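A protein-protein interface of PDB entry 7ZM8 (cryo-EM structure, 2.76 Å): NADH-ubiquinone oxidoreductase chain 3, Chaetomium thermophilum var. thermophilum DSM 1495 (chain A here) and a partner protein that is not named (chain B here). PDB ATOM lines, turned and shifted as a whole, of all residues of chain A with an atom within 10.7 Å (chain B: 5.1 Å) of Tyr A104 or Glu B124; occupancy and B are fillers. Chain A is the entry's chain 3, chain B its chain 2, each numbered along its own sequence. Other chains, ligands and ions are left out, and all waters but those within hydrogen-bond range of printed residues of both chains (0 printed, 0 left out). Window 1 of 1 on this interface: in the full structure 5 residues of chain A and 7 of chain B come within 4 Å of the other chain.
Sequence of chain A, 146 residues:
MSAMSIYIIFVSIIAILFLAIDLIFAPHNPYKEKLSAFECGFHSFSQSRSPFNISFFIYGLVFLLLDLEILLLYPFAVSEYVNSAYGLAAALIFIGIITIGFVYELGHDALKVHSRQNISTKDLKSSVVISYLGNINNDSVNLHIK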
ATOM      1  N   ILE A  58      -0.104 -22.085 -18.362  1.00  0.00           N
ATOM      2  CA  ILE A  58      -1.165 -22.833 -17.700  1.00  0.00           C
ATOM      3  C   ILE A  58      -2.124 -23.433 -18.717  1.00  0.00           C
ATOM      4  O   ILE A  58      -2.648 -24.534 -18.521  1.00  0.00           O
ATOM      5  CB  ILE A  58      -1.892 -21.926 -16.693  1.00  0.00           C
ATOM      6  CG1 ILE A  58      -0.876 -21.216 -15.794  1.00  0.00           C
ATOM      7  CG2 ILE A  58      -2.900 -22.719 -15.877  1.00  0.00           C
ATOM      8  CD1 ILE A  58       0.073 -22.135 -15.102  1.00  0.00           C
ATOM      9  N   LEU A  61      -0.459 -26.461 -19.971  1.00  0.00           N
ATOM     10  CA  LEU A  61      -0.284 -27.402 -18.875  1.00  0.00           C
ATOM     11  C   LEU A  61      -1.566 -28.168 -18.595  1.00  0.00           C
ATOM     12  O   LEU A  61      -1.569 -29.401 -18.527  1.00  0.00           O
ATOM     13  CB  LEU A  61       0.146 -26.637 -17.629  1.00  0.00           C
ATOM     14  CG  LEU A  61       0.450 -27.422 -16.363  1.00  0.00           C
ATOM     15  CD1 LEU A  61       1.622 -28.342 -16.577  1.00  0.00           C
ATOM     16  CD2 LEU A  61       0.686 -26.467 -15.222  1.00  0.00           C
ATOM     17  N   VAL A  62      -2.668 -27.446 -18.409  1.00  0.00           N
ATOM     18  CA  VAL A  62      -3.924 -28.085 -18.061  1.00  0.00           C
ATOM     19  C   VAL A  62      -4.491 -28.843 -19.248  1.00  0.00           C
ATOM     20  O   VAL A  62      -5.122 -29.892 -19.079  1.00  0.00           O
ATOM     21  CB  VAL A  62      -4.905 -27.036 -17.520  1.00  0.00           C
ATOM     22  CG1 VAL A  62      -6.164 -27.706 -17.045  1.00  0.00           C
ATOM     23  CG2 VAL A  62      -4.255 -26.268 -16.386  1.00  0.00           C
ATOM     24  N   LEU A  65      -2.588 -32.261 -19.413  1.00  0.00           N
ATOM     25  CA  LEU A  65      -2.972 -33.235 -18.406  1.00  0.00           C
ATOM     26  C   LEU A  65      -4.382 -33.762 -18.633  1.00  0.00           C
ATOM     27  O   LEU A  65      -4.608 -34.973 -18.557  1.00  0.00           O
ATOM     28  CB  LEU A  65      -2.832 -32.620 -17.017  1.00  0.00           C
ATOM     29  CG  LEU A  65      -1.382 -32.360 -16.613  1.00  0.00           C
ATOM     30  CD1 LEU A  65      -1.312 -31.895 -15.179  1.00  0.00           C
ATOM     31  CD2 LEU A  65      -0.510 -33.586 -16.826  1.00  0.00           C
ATOM     32  N   LEU A  66      -5.339 -32.877 -18.922  1.00  0.00           N
ATOM     33  CA  LEU A  66      -6.704 -33.319 -19.196  1.00  0.00           C
ATOM     34  C   LEU A  66      -6.808 -34.079 -20.510  1.00  0.00           C
ATOM     35  O   LEU A  66      -7.632 -34.989 -20.628  1.00  0.00           O
ATOM     36  CB  LEU A  66      -7.663 -32.130 -19.204  1.00  0.00           C
ATOM     37  CG  LEU A  66      -8.230 -31.601 -17.886  1.00  0.00           C
ATOM     38  CD1 LEU A  66      -9.097 -32.656 -17.225  1.00  0.00           C
ATOM     39  CD2 LEU A  66      -7.142 -31.160 -16.941  1.00  0.00           C
ATOM     40  N   GLY A  96     -13.082 -39.631 -10.573  1.00  0.00           N
ATOM     41  CA  GLY A  96     -13.091 -38.831  -9.341  1.00  0.00           C
ATOM     42  C   GLY A  96     -11.751 -38.222  -8.969  1.00  0.00           C
ATOM     43  O   GLY A  96     -11.753 -37.061  -8.565  1.00  0.00           O
ATOM     44  N   ILE A  97     -10.658 -38.975  -9.094  1.00  0.00           N
ATOM     45  CA  ILE A  97      -9.298 -38.433  -8.797  1.00  0.00           C
ATOM     46  C   ILE A  97      -8.993 -37.248  -9.729  1.00  0.00           C
ATOM     47  O   ILE A  97      -8.567 -36.201  -9.221  1.00  0.00           O
ATOM     48  CB  ILE A  97      -8.237 -39.552  -8.850  1.00  0.00           C
ATOM     49  CG1 ILE A  97      -8.585 -40.691  -7.889  1.00  0.00           C
ATOM     50  CG2 ILE A  97      -6.842 -39.005  -8.591  1.00  0.00           C
ATOM     51  CD1 ILE A  97      -7.778 -41.950  -8.097  1.00  0.00           C
ATOM     52  N   ILE A  98      -9.209 -37.406 -11.036  1.00  0.00           N
ATOM     53  CA  ILE A  98      -8.929 -36.319 -12.018  1.00  0.00           C
ATOM     54  C   ILE A  98      -9.858 -35.118 -11.782  1.00  0.00           C
ATOM     55  O   ILE A  98      -9.390 -33.982 -11.953  1.00  0.00           O
ATOM     56  CB  ILE A  98      -8.891 -36.845 -13.472  1.00  0.00           C
ATOM     57  CG1 ILE A  98     -10.278 -37.115 -14.058  1.00  0.00           C
ATOM     58  CG2 ILE A  98      -7.993 -38.067 -13.567  1.00  0.00           C
ATOM     59  CD1 ILE A  98     -10.261 -37.988 -15.292  1.00  0.00           C
ATOM     60  N   THR A  99     -11.120 -35.353 -11.426  1.00  0.00           N
ATOM     61  CA  THR A  99     -12.054 -34.244 -11.105  1.00  0.00           C
ATOM     62  C   THR A  99     -11.525 -33.419  -9.923  1.00  0.00           C
ATOM     63  O   THR A  99     -11.562 -32.191 -10.012  1.00  0.00           O
ATOM     64  CB  THR A  99     -13.465 -34.788 -10.862  1.00  0.00           C
ATOM     65  OG1 THR A  99     -13.827 -35.569 -11.999  1.00  0.00           O
ATOM     66  CG2 THR A  99     -14.489 -33.697 -10.653  1.00  0.00           C
ATOM     67  N   ILE A 100     -11.056 -34.074  -8.864  1.00  0.00           N
ATOM     68  CA  ILE A 100     -10.534 -33.371  -7.668  1.00  0.00           C
ATOM     69  C   ILE A 100      -9.398 -32.424  -8.101  1.00  0.00           C
ATOM     70  O   ILE A 100      -9.345 -31.301  -7.582  1.00  0.00           O
ATOM     71  CB  ILE A 100     -10.136 -34.412  -6.603  1.00  0.00           C
ATOM     72  CG1 ILE A 100     -11.365 -35.055  -5.962  1.00  0.00           C
ATOM     73  CG2 ILE A 100      -9.222 -33.814  -5.549  1.00  0.00           C
ATOM     74  CD1 ILE A 100     -11.035 -36.097  -4.924  1.00  0.00           C
ATOM     75  N   GLY A 101      -8.524 -32.833  -9.021  1.00  0.00           N
ATOM     76  CA  GLY A 101      -7.473 -31.940  -9.538  1.00  0.00           C
ATOM     77  C   GLY A 101      -8.043 -30.752 -10.280  1.00  0.00           C
ATOM     78  O   GLY A 101      -7.441 -29.681 -10.219  1.00  0.00           O
ATOM     79  N   PHE A 102      -9.117 -30.948 -11.035  1.00  0.00           N
ATOM     80  CA  PHE A 102      -9.819 -29.860 -11.753  1.00  0.00           C
ATOM     81  C   PHE A 102     -10.425 -28.876 -10.749  1.00  0.00           C
ATOM     82  O   PHE A 102     -10.424 -27.682 -11.007  1.00  0.00           O
ATOM     83  CB  PHE A 102     -10.850 -30.505 -12.678  1.00  0.00           C
ATOM     84  CG  PHE A 102     -11.630 -29.572 -13.565  1.00  0.00           C
ATOM     85  CD1 PHE A 102     -11.035 -28.972 -14.661  1.00  0.00           C
ATOM     86  CD2 PHE A 102     -12.970 -29.325 -13.325  1.00  0.00           C
ATOM     87  CE1 PHE A 102     -11.755 -28.123 -15.485  1.00  0.00           C
ATOM     88  CE2 PHE A 102     -13.690 -28.482 -14.154  1.00  0.00           C
ATOM     89  CZ  PHE A 102     -13.080 -27.884 -15.229  1.00  0.00           C
ATOM     90  N   VAL A 103     -10.978 -29.371  -9.651  1.00  0.00           N
ATOM     91  CA  VAL A 103     -11.614 -28.485  -8.637  1.00  0.00           C
ATOM     92  C   VAL A 103     -10.509 -27.637  -8.000  1.00  0.00           C
ATOM     93  O   VAL A 103     -10.816 -26.553  -7.494  1.00  0.00           O
ATOM     94  CB  VAL A 103     -12.509 -29.213  -7.613  1.00  0.00           C
ATOM     95  CG1 VAL A 103     -13.393 -30.276  -8.237  1.00  0.00           C
ATOM     96  CG2 VAL A 103     -11.744 -29.749  -6.422  1.00  0.00           C
ATOM     97  N   TYR A 104      -9.273 -28.128  -8.028  1.00  0.00           N
ATOM     98  CA  TYR A 104      -8.134 -27.393  -7.436  1.00  0.00           C
ATOM     99  C   TYR A 104      -7.750 -26.223  -8.328  1.00  0.00           C
ATOM    100  O   TYR A 104      -7.400 -25.174  -7.797  1.00  0.00           O
ATOM    101  CB  TYR A 104      -6.955 -28.350  -7.261  1.00  0.00           C
ATOM    102  CG  TYR A 104      -5.661 -27.722  -6.813  1.00  0.00           C
ATOM    103  CD1 TYR A 104      -5.389 -27.531  -5.470  1.00  0.00           C
ATOM    104  CD2 TYR A 104      -4.701 -27.338  -7.731  1.00  0.00           C
ATOM    105  CE1 TYR A 104      -4.203 -26.957  -5.051  1.00  0.00           C
ATOM    106  CE2 TYR A 104      -3.512 -26.756  -7.328  1.00  0.00           C
ATOM    107  CZ  TYR A 104      -3.259 -26.572  -5.983  1.00  0.00           C
ATOM    108  OH  TYR A 104      -2.083 -26.013  -5.584  1.00  0.00           O
ATOM    109  N   GLU A 105      -7.847 -26.398  -9.646  1.00  0.00           N
ATOM    110  CA  GLU A 105      -7.485 -25.316 -10.594  1.00  0.00           C
ATOM    111  C   GLU A 105      -8.666 -24.367 -10.669  1.00  0.00           C
ATOM    112  O   GLU A 105      -8.470 -23.180 -10.936  1.00  0.00           O
ATOM    113  CB  GLU A 105      -7.057 -25.889 -11.936  1.00  0.00           C
ATOM    114  CG  GLU A 105      -8.092 -26.731 -12.637  1.00  0.00           C
ATOM    115  CD  GLU A 105      -7.422 -27.467 -13.773  1.00  0.00           C
ATOM    116  OE1 GLU A 105      -6.265 -27.125 -14.051  1.00  0.00           O
ATOM    117  OE2 GLU A 105      -8.033 -28.379 -14.353  1.00  0.00           O
ATOM    118  N   LEU A 106      -9.857 -24.897 -10.463  1.00  0.00           N
ATOM    119  CA  LEU A 106     -10.998 -24.005 -10.311  1.00  0.00           C
ATOM    120  C   LEU A 106     -10.909 -23.223  -9.010  1.00  0.00           C
ATOM    121  O   LEU A 106     -11.151 -22.012  -8.989  1.00  0.00           O
ATOM    122  CB  LEU A 106     -12.296 -24.801 -10.361  1.00  0.00           C
ATOM    123  CG  LEU A 106     -12.674 -25.358 -11.724  1.00  0.00           C
ATOM    124  CD1 LEU A 106     -14.107 -25.855 -11.701  1.00  0.00           C
ATOM    125  CD2 LEU A 106     -12.481 -24.300 -12.794  1.00  0.00           C
ATOM    126  N   GLY A 107     -10.458 -23.856  -7.938  1.00  0.00           N
ATOM    127  CA  GLY A 107     -10.370 -23.203  -6.628  1.00  0.00           C
ATOM    128  C   GLY A 107      -9.297 -22.150  -6.572  1.00  0.00           C
ATOM    129  O   GLY A 107      -9.496 -21.170  -5.870  1.00  0.00           O
ATOM    130  N   HIS A 108      -8.168 -22.348  -7.233  1.00  0.00           N
ATOM    131  CA  HIS A 108      -7.060 -21.379  -7.089  1.00  0.00           C
ATOM    132  C   HIS A 108      -7.071 -20.435  -8.280  1.00  0.00           C
ATOM    133  O   HIS A 108      -6.134 -19.630  -8.399  1.00  0.00           O
ATOM    134  CB  HIS A 108      -5.738 -22.120  -6.901  1.00  0.00           C
ATOM    135  CG  HIS A 108      -5.631 -22.849  -5.607  1.00  0.00           C
ATOM    136  ND1 HIS A 108      -4.686 -22.530  -4.663  1.00  0.00           N
ATOM    137  CD2 HIS A 108      -6.349 -23.867  -5.093  1.00  0.00           C
ATOM    138  CE1 HIS A 108      -4.829 -23.320  -3.621  1.00  0.00           C
ATOM    139  NE2 HIS A 108      -5.838 -24.146  -3.863  1.00  0.00           N
ATOM    140  N   ASP A 109      -8.099 -20.521  -9.114  1.00  0.00           N
ATOM    141  CA  ASP A 109      -8.147 -19.732 -10.366  1.00  0.00           C
ATOM    142  C   ASP A 109      -6.776 -19.832 -11.021  1.00  0.00           C
ATOM    143  O   ASP A 109      -6.212 -18.800 -11.375  1.00  0.00           O
ATOM    144  CB  ASP A 109      -8.628 -18.304 -10.134  1.00  0.00           C
ATOM    145  CG  ASP A 109      -8.966 -17.552 -11.412  1.00  0.00           C
ATOM    146  OD1 ASP A 109      -9.401 -18.203 -12.386  1.00  0.00           O
ATOM    147  OD2 ASP A 109      -8.775 -16.321 -11.432  1.00  0.00           O
ATOM    148  N   ALA A 110      -6.242 -21.046 -11.118  1.00  0.00           N
ATOM    149  CA  ALA A 110      -4.923 -21.203 -11.712  1.00  0.00           C
ATOM    150  C   ALA A 110      -4.902 -20.693 -13.138  1.00  0.00           C
ATOM    151  O   ALA A 110      -3.896 -20.134 -13.587  1.00  0.00           O
ATOM    152  CB  ALA A 110      -4.495 -22.665 -11.668  1.00  0.00           C
ATOM    153  N   LEU A 111      -6.011 -20.867 -13.854  1.00  0.00           N
ATOM    154  CA  LEU A 111      -6.120 -20.386 -15.220  1.00  0.00           C
ATOM    155  C   LEU A 111      -6.061 -18.867 -15.269  1.00  0.00           C
ATOM    156  O   LEU A 111      -5.868 -18.298 -16.347  1.00  0.00           O
ATOM    157  CB  LEU A 111      -7.429 -20.895 -15.832  1.00  0.00           C
ATOM    158  CG  LEU A 111      -7.541 -22.313 -16.424  1.00  0.00           C
ATOM    159  CD1 LEU A 111      -6.651 -22.539 -17.626  1.00  0.00           C
ATOM    160  CD2 LEU A 111      -7.284 -23.382 -15.367  1.00  0.00           C
ATOM    161  N   LYS A 112      -6.219 -18.208 -14.118  1.00  0.00           N
ATOM    162  CA  LYS A 112      -6.124 -16.754 -13.991  1.00  0.00           C
ATOM    163  C   LYS A 112      -7.023 -16.066 -15.006  1.00  0.00           C
ATOM    164  O   LYS A 112      -6.613 -15.166 -15.741  1.00  0.00           O
ATOM    165  CB  LYS A 112      -4.677 -16.279 -14.116  1.00  0.00           C
ATOM    166  CG  LYS A 112      -3.814 -16.735 -12.961  1.00  0.00           C
ATOM    167  CD  LYS A 112      -2.627 -15.838 -12.746  1.00  0.00           C
ATOM    168  CE  LYS A 112      -1.743 -16.389 -11.649  1.00  0.00           C
ATOM    169  NZ  LYS A 112      -2.329 -16.193 -10.303  1.00  0.00           N
ATOM    170  N   LEU B  10      -6.478 -32.468  -0.249  1.00  0.00           N
ATOM    171  CA  LEU B  10      -6.479 -31.770  -1.552  1.00  0.00           C
ATOM    172  C   LEU B  10      -7.780 -30.992  -1.722  1.00  0.00           C
ATOM    173  O   LEU B  10      -7.698 -29.836  -2.119  1.00  0.00           O
ATOM    174  CB  LEU B  10      -6.332 -32.832  -2.640  1.00  0.00           C
ATOM    175  CG  LEU B  10      -6.118 -32.325  -4.064  1.00  0.00           C
ATOM    176  CD1 LEU B  10      -5.225 -31.098  -4.095  1.00  0.00           C
ATOM    177  CD2 LEU B  10      -5.530 -33.425  -4.924  1.00  0.00           C
ATOM    178  N   THR B  13      -7.773 -27.998   0.579  1.00  0.00           N
ATOM    179  CA  THR B  13      -6.743 -27.026   0.145  1.00  0.00           C
ATOM    180  C   THR B  13      -7.209 -26.348  -1.139  1.00  0.00           C
ATOM    181  O   THR B  13      -6.883 -25.171  -1.322  1.00  0.00           O
ATOM    182  CB  THR B  13      -5.415 -27.768  -0.026  1.00  0.00           C
ATOM    183  OG1 THR B  13      -5.036 -28.263   1.258  1.00  0.00           O
ATOM    184  CG2 THR B  13      -4.303 -26.924  -0.605  1.00  0.00           C
ATOM    185  N   SER B  14      -7.950 -27.062  -1.978  1.00  0.00           N
ATOM    186  CA  SER B  14      -8.424 -26.533  -3.281  1.00  0.00           C
ATOM    187  C   SER B  14      -9.389 -25.371  -3.085  1.00  0.00           C
ATOM    188  O   SER B  14      -9.336 -24.442  -3.884  1.00  0.00           O
ATOM    189  CB  SER B  14      -9.096 -27.626  -4.036  1.00  0.00           C
ATOM    190  OG  SER B  14      -8.205 -28.691  -4.304  1.00  0.00           O
ATOM    191  N   ILE B 122       3.228 -22.008   2.906  1.00  0.00           N
ATOM    192  CA  ILE B 122       2.976 -22.850   1.696  1.00  0.00           C
ATOM    193  C   ILE B 122       1.848 -23.821   2.040  1.00  0.00           C
ATOM    194  O   ILE B 122       2.087 -24.740   2.831  1.00  0.00           O
ATOM    195  CB  ILE B 122       4.253 -23.555   1.198  1.00  0.00           C
ATOM    196  CG1 ILE B 122       5.471 -22.632   1.278  1.00  0.00           C
ATOM    197  CG2 ILE B 122       4.046 -24.100  -0.205  1.00  0.00           C
ATOM    198  CD1 ILE B 122       6.712 -23.185   0.621  1.00  0.00           C
ATOM    199  N   ILE B 123       0.666 -23.611   1.473  1.00  0.00           N
ATOM    200  CA  ILE B 123      -0.536 -24.431   1.804  1.00  0.00           C
ATOM    201  C   ILE B 123      -0.360 -25.865   1.312  1.00  0.00           C
ATOM    202  O   ILE B 123      -0.843 -26.774   1.998  1.00  0.00           O
ATOM    203  CB  ILE B 123      -1.795 -23.758   1.216  1.00  0.00           C
ATOM    204  CG1 ILE B 123      -1.670 -22.232   1.211  1.00  0.00           C
ATOM    205  CG2 ILE B 123      -3.054 -24.214   1.928  1.00  0.00           C
ATOM    206  CD1 ILE B 123      -2.771 -21.529   0.451  1.00  0.00           C
ATOM    207  N   GLU B 124       0.272 -26.054   0.158  1.00  0.00           N
ATOM    208  CA  GLU B 124       0.350 -27.407  -0.452  1.00  0.00           C
ATOM    209  C   GLU B 124       1.633 -28.133  -0.047  1.00  0.00           C
ATOM    210  O   GLU B 124       1.869 -29.212  -0.582  1.00  0.00           O
ATOM    211  CB  GLU B 124       0.268 -27.299  -1.976  1.00  0.00           C
ATOM    212  CG  GLU B 124      -1.048 -26.732  -2.479  1.00  0.00           C
ATOM    213  CD  GLU B 124      -1.210 -25.224  -2.387  1.00  0.00           C
ATOM    214  OE1 GLU B 124      -0.201 -24.529  -2.152  1.00  0.00           O
ATOM    215  OE2 GLU B 124      -2.348 -24.748  -2.540  1.00  0.00           O
ATOM    216  N   TYR B 125       2.409 -27.571   0.869  1.00  0.00           N
ATOM    217  CA  TYR B 125       3.631 -28.265   1.345  1.00  0.00           C
ATOM    218  C   TYR B 125       3.292 -29.566   2.087  1.00  0.00           C
ATOM    219  O   TYR B 125       3.925 -30.585   1.755  1.00  0.00           O
ATOM    220  CB  TYR B 125       4.533 -27.320   2.142  1.00  0.00           C
ATOM    221  CG  TYR B 125       5.850 -27.915   2.575  1.00  0.00           C
ATOM    222  CD1 TYR B 125       6.958 -27.875   1.746  1.00  0.00           C
ATOM    223  CD2 TYR B 125       5.992 -28.516   3.815  1.00  0.00           C
ATOM    224  CE1 TYR B 125       8.170 -28.419   2.133  1.00  0.00           C
ATOM    225  CE2 TYR B 125       7.197 -29.065   4.217  1.00  0.00           C
ATOM    226  CZ  TYR B 125       8.293 -29.015   3.374  1.00  0.00           C
ATOM    227  OH  TYR B 125       9.485 -29.549   3.765  1.00  0.00           O
ATOM    228  N   PRO B 126       2.318 -29.623   3.025  1.00  0.00           N
ATOM    229  CA  PRO B 126       1.972 -30.890   3.670  1.00  0.00           C
ATOM    230  C   PRO B 126       1.422 -31.883   2.640  1.00  0.00           C
ATOM    231  O   PRO B 126       1.621 -33.053   2.819  1.00  0.00           O
ATOM    232  CB  PRO B 126       0.910 -30.463   4.688  1.00  0.00           C
ATOM    233  CG  PRO B 126       0.330 -29.202   4.122  1.00  0.00           C
ATOM    234  CD  PRO B 126       1.545 -28.501   3.568  1.00  0.00           C
ATOM    235  N   LEU B 127       0.788 -31.388   1.583  1.00  0.00           N
ATOM    236  CA  LEU B 127       0.174 -32.207   0.547  1.00  0.00           C
ATOM    237  C   LEU B 127       1.225 -32.907  -0.302  1.00  0.00           C
ATOM    238  O   LEU B 127       1.086 -34.086  -0.636  1.00  0.00           O
ATOM    239  CB  LEU B 127      -0.727 -31.331  -0.321  1.00  0.00           C
ATOM    240  CG  LEU B 127      -1.500 -31.975  -1.468  1.00  0.00           C
ATOM    241  CD1 LEU B 127      -2.403 -33.071  -0.958  1.00  0.00           C
ATOM    242  CD2 LEU B 127      -2.292 -30.925  -2.194  1.00  0.00           C
ATOM    243  N   ILE B 128       2.290 -32.188  -0.663  1.00  0.00           N
ATOM    244  CA  ILE B 128       3.275 -32.726  -1.592  1.00  0.00           C
ATOM    245  C   ILE B 128       4.182 -33.740  -0.908  1.00  0.00           C
ATOM    246  O   ILE B 128       4.640 -34.691  -1.547  1.00  0.00           O
ATOM    247  CB  ILE B 128       4.060 -31.573  -2.243  1.00  0.00           C
ATOM    248  CG1 ILE B 128       3.092 -30.669  -3.001  1.00  0.00           C
ATOM    249  CG2 ILE B 128       5.102 -32.100  -3.207  1.00  0.00           C
ATOM    250  CD1 ILE B 128       3.752 -29.697  -3.933  1.00  0.00           C
ATOM    251  N   ILE B 165       9.711 -25.517  -4.526  1.00  0.00           N
ATOM    252  CA  ILE B 165       8.522 -24.904  -3.855  1.00  0.00           C
ATOM    253  C   ILE B 165       8.798 -23.505  -3.293  1.00  0.00           C
ATOM    254  O   ILE B 165       7.848 -22.704  -3.235  1.00  0.00           O
ATOM    255  CB  ILE B 165       7.865 -25.886  -2.856  1.00  0.00           C
ATOM    256  CG1 ILE B 165       6.345 -25.717  -2.809  1.00  0.00           C
ATOM    257  CG2 ILE B 165       8.500 -25.821  -1.477  1.00  0.00           C
ATOM    258  CD1 ILE B 165       5.612 -26.891  -2.205  1.00  0.00           C
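A ring nitrogen (NE2) of His A108 sits at hydrogen-bond distance from the backbone carbonyl oxygen (O) of Thr B13.
OH of Tyr A104 lies within hydrogen-bond range of OE2 of Glu B124, 3.3 Å away.
The backbone carbonyl oxygen of Leu B10 is in hydrogen-bond range of the side-chain hydroxyl of Ser B14.
Among the printed residues, pairs that only touch across the chains: Ile A100 with Leu B10, Tyr A104 with Leu B10, Tyr A104 with Ser B14, Gly A107 with Ser B14, His A108 with Ser B14 and His A108 with Glu B124.
Gly A101 touches none of the printed residues of chain B.
Of the printed residues of chain B, Tyr A104 touches Leu B10 (3.8 Å), Ser B14 (3.2 Å) and Glu B124 (3.3 Å).
Of the printed residues of chain B, Gly A107 touches Ser B14 (3.2 Å).
Printed residues of chain B within 4 Å of His A108: Thr B13, Ser B14 and Glu B124.
Of the printed residues of chain A, Leu B10 touches Ile A100 and Tyr A104.
Of chain A, only His A108 comes within 4 Å of Thr B13.
Ile B123 touches none of the printed residues of chain A.
No residue of chain A comes within 4 Å of Pro B126.
Leu B127 touches none of the printed residues of chain A.
The nearest residue of chain A that does not touch Glu B124 is Gly A107 (8.4 Å).
The nearest printed residue of chain A that does not touch Ser B14 is Val A103 (4.01 Å).
Printed residues of chain A that touch a printed residue of chain B: Ile A100, Tyr A104, Gly A107 and His A108.
Printed residues of chain B that touch a printed residue of chain A: Leu B10, Thr B13, Ser B14 and Glu B124.
Hydrophobic or aromatic side chains of chain B that line the printed part of chain A: Leu B10.
Along chain B the printed residues that touch a printed residue of chain A span positions 10 to 124.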
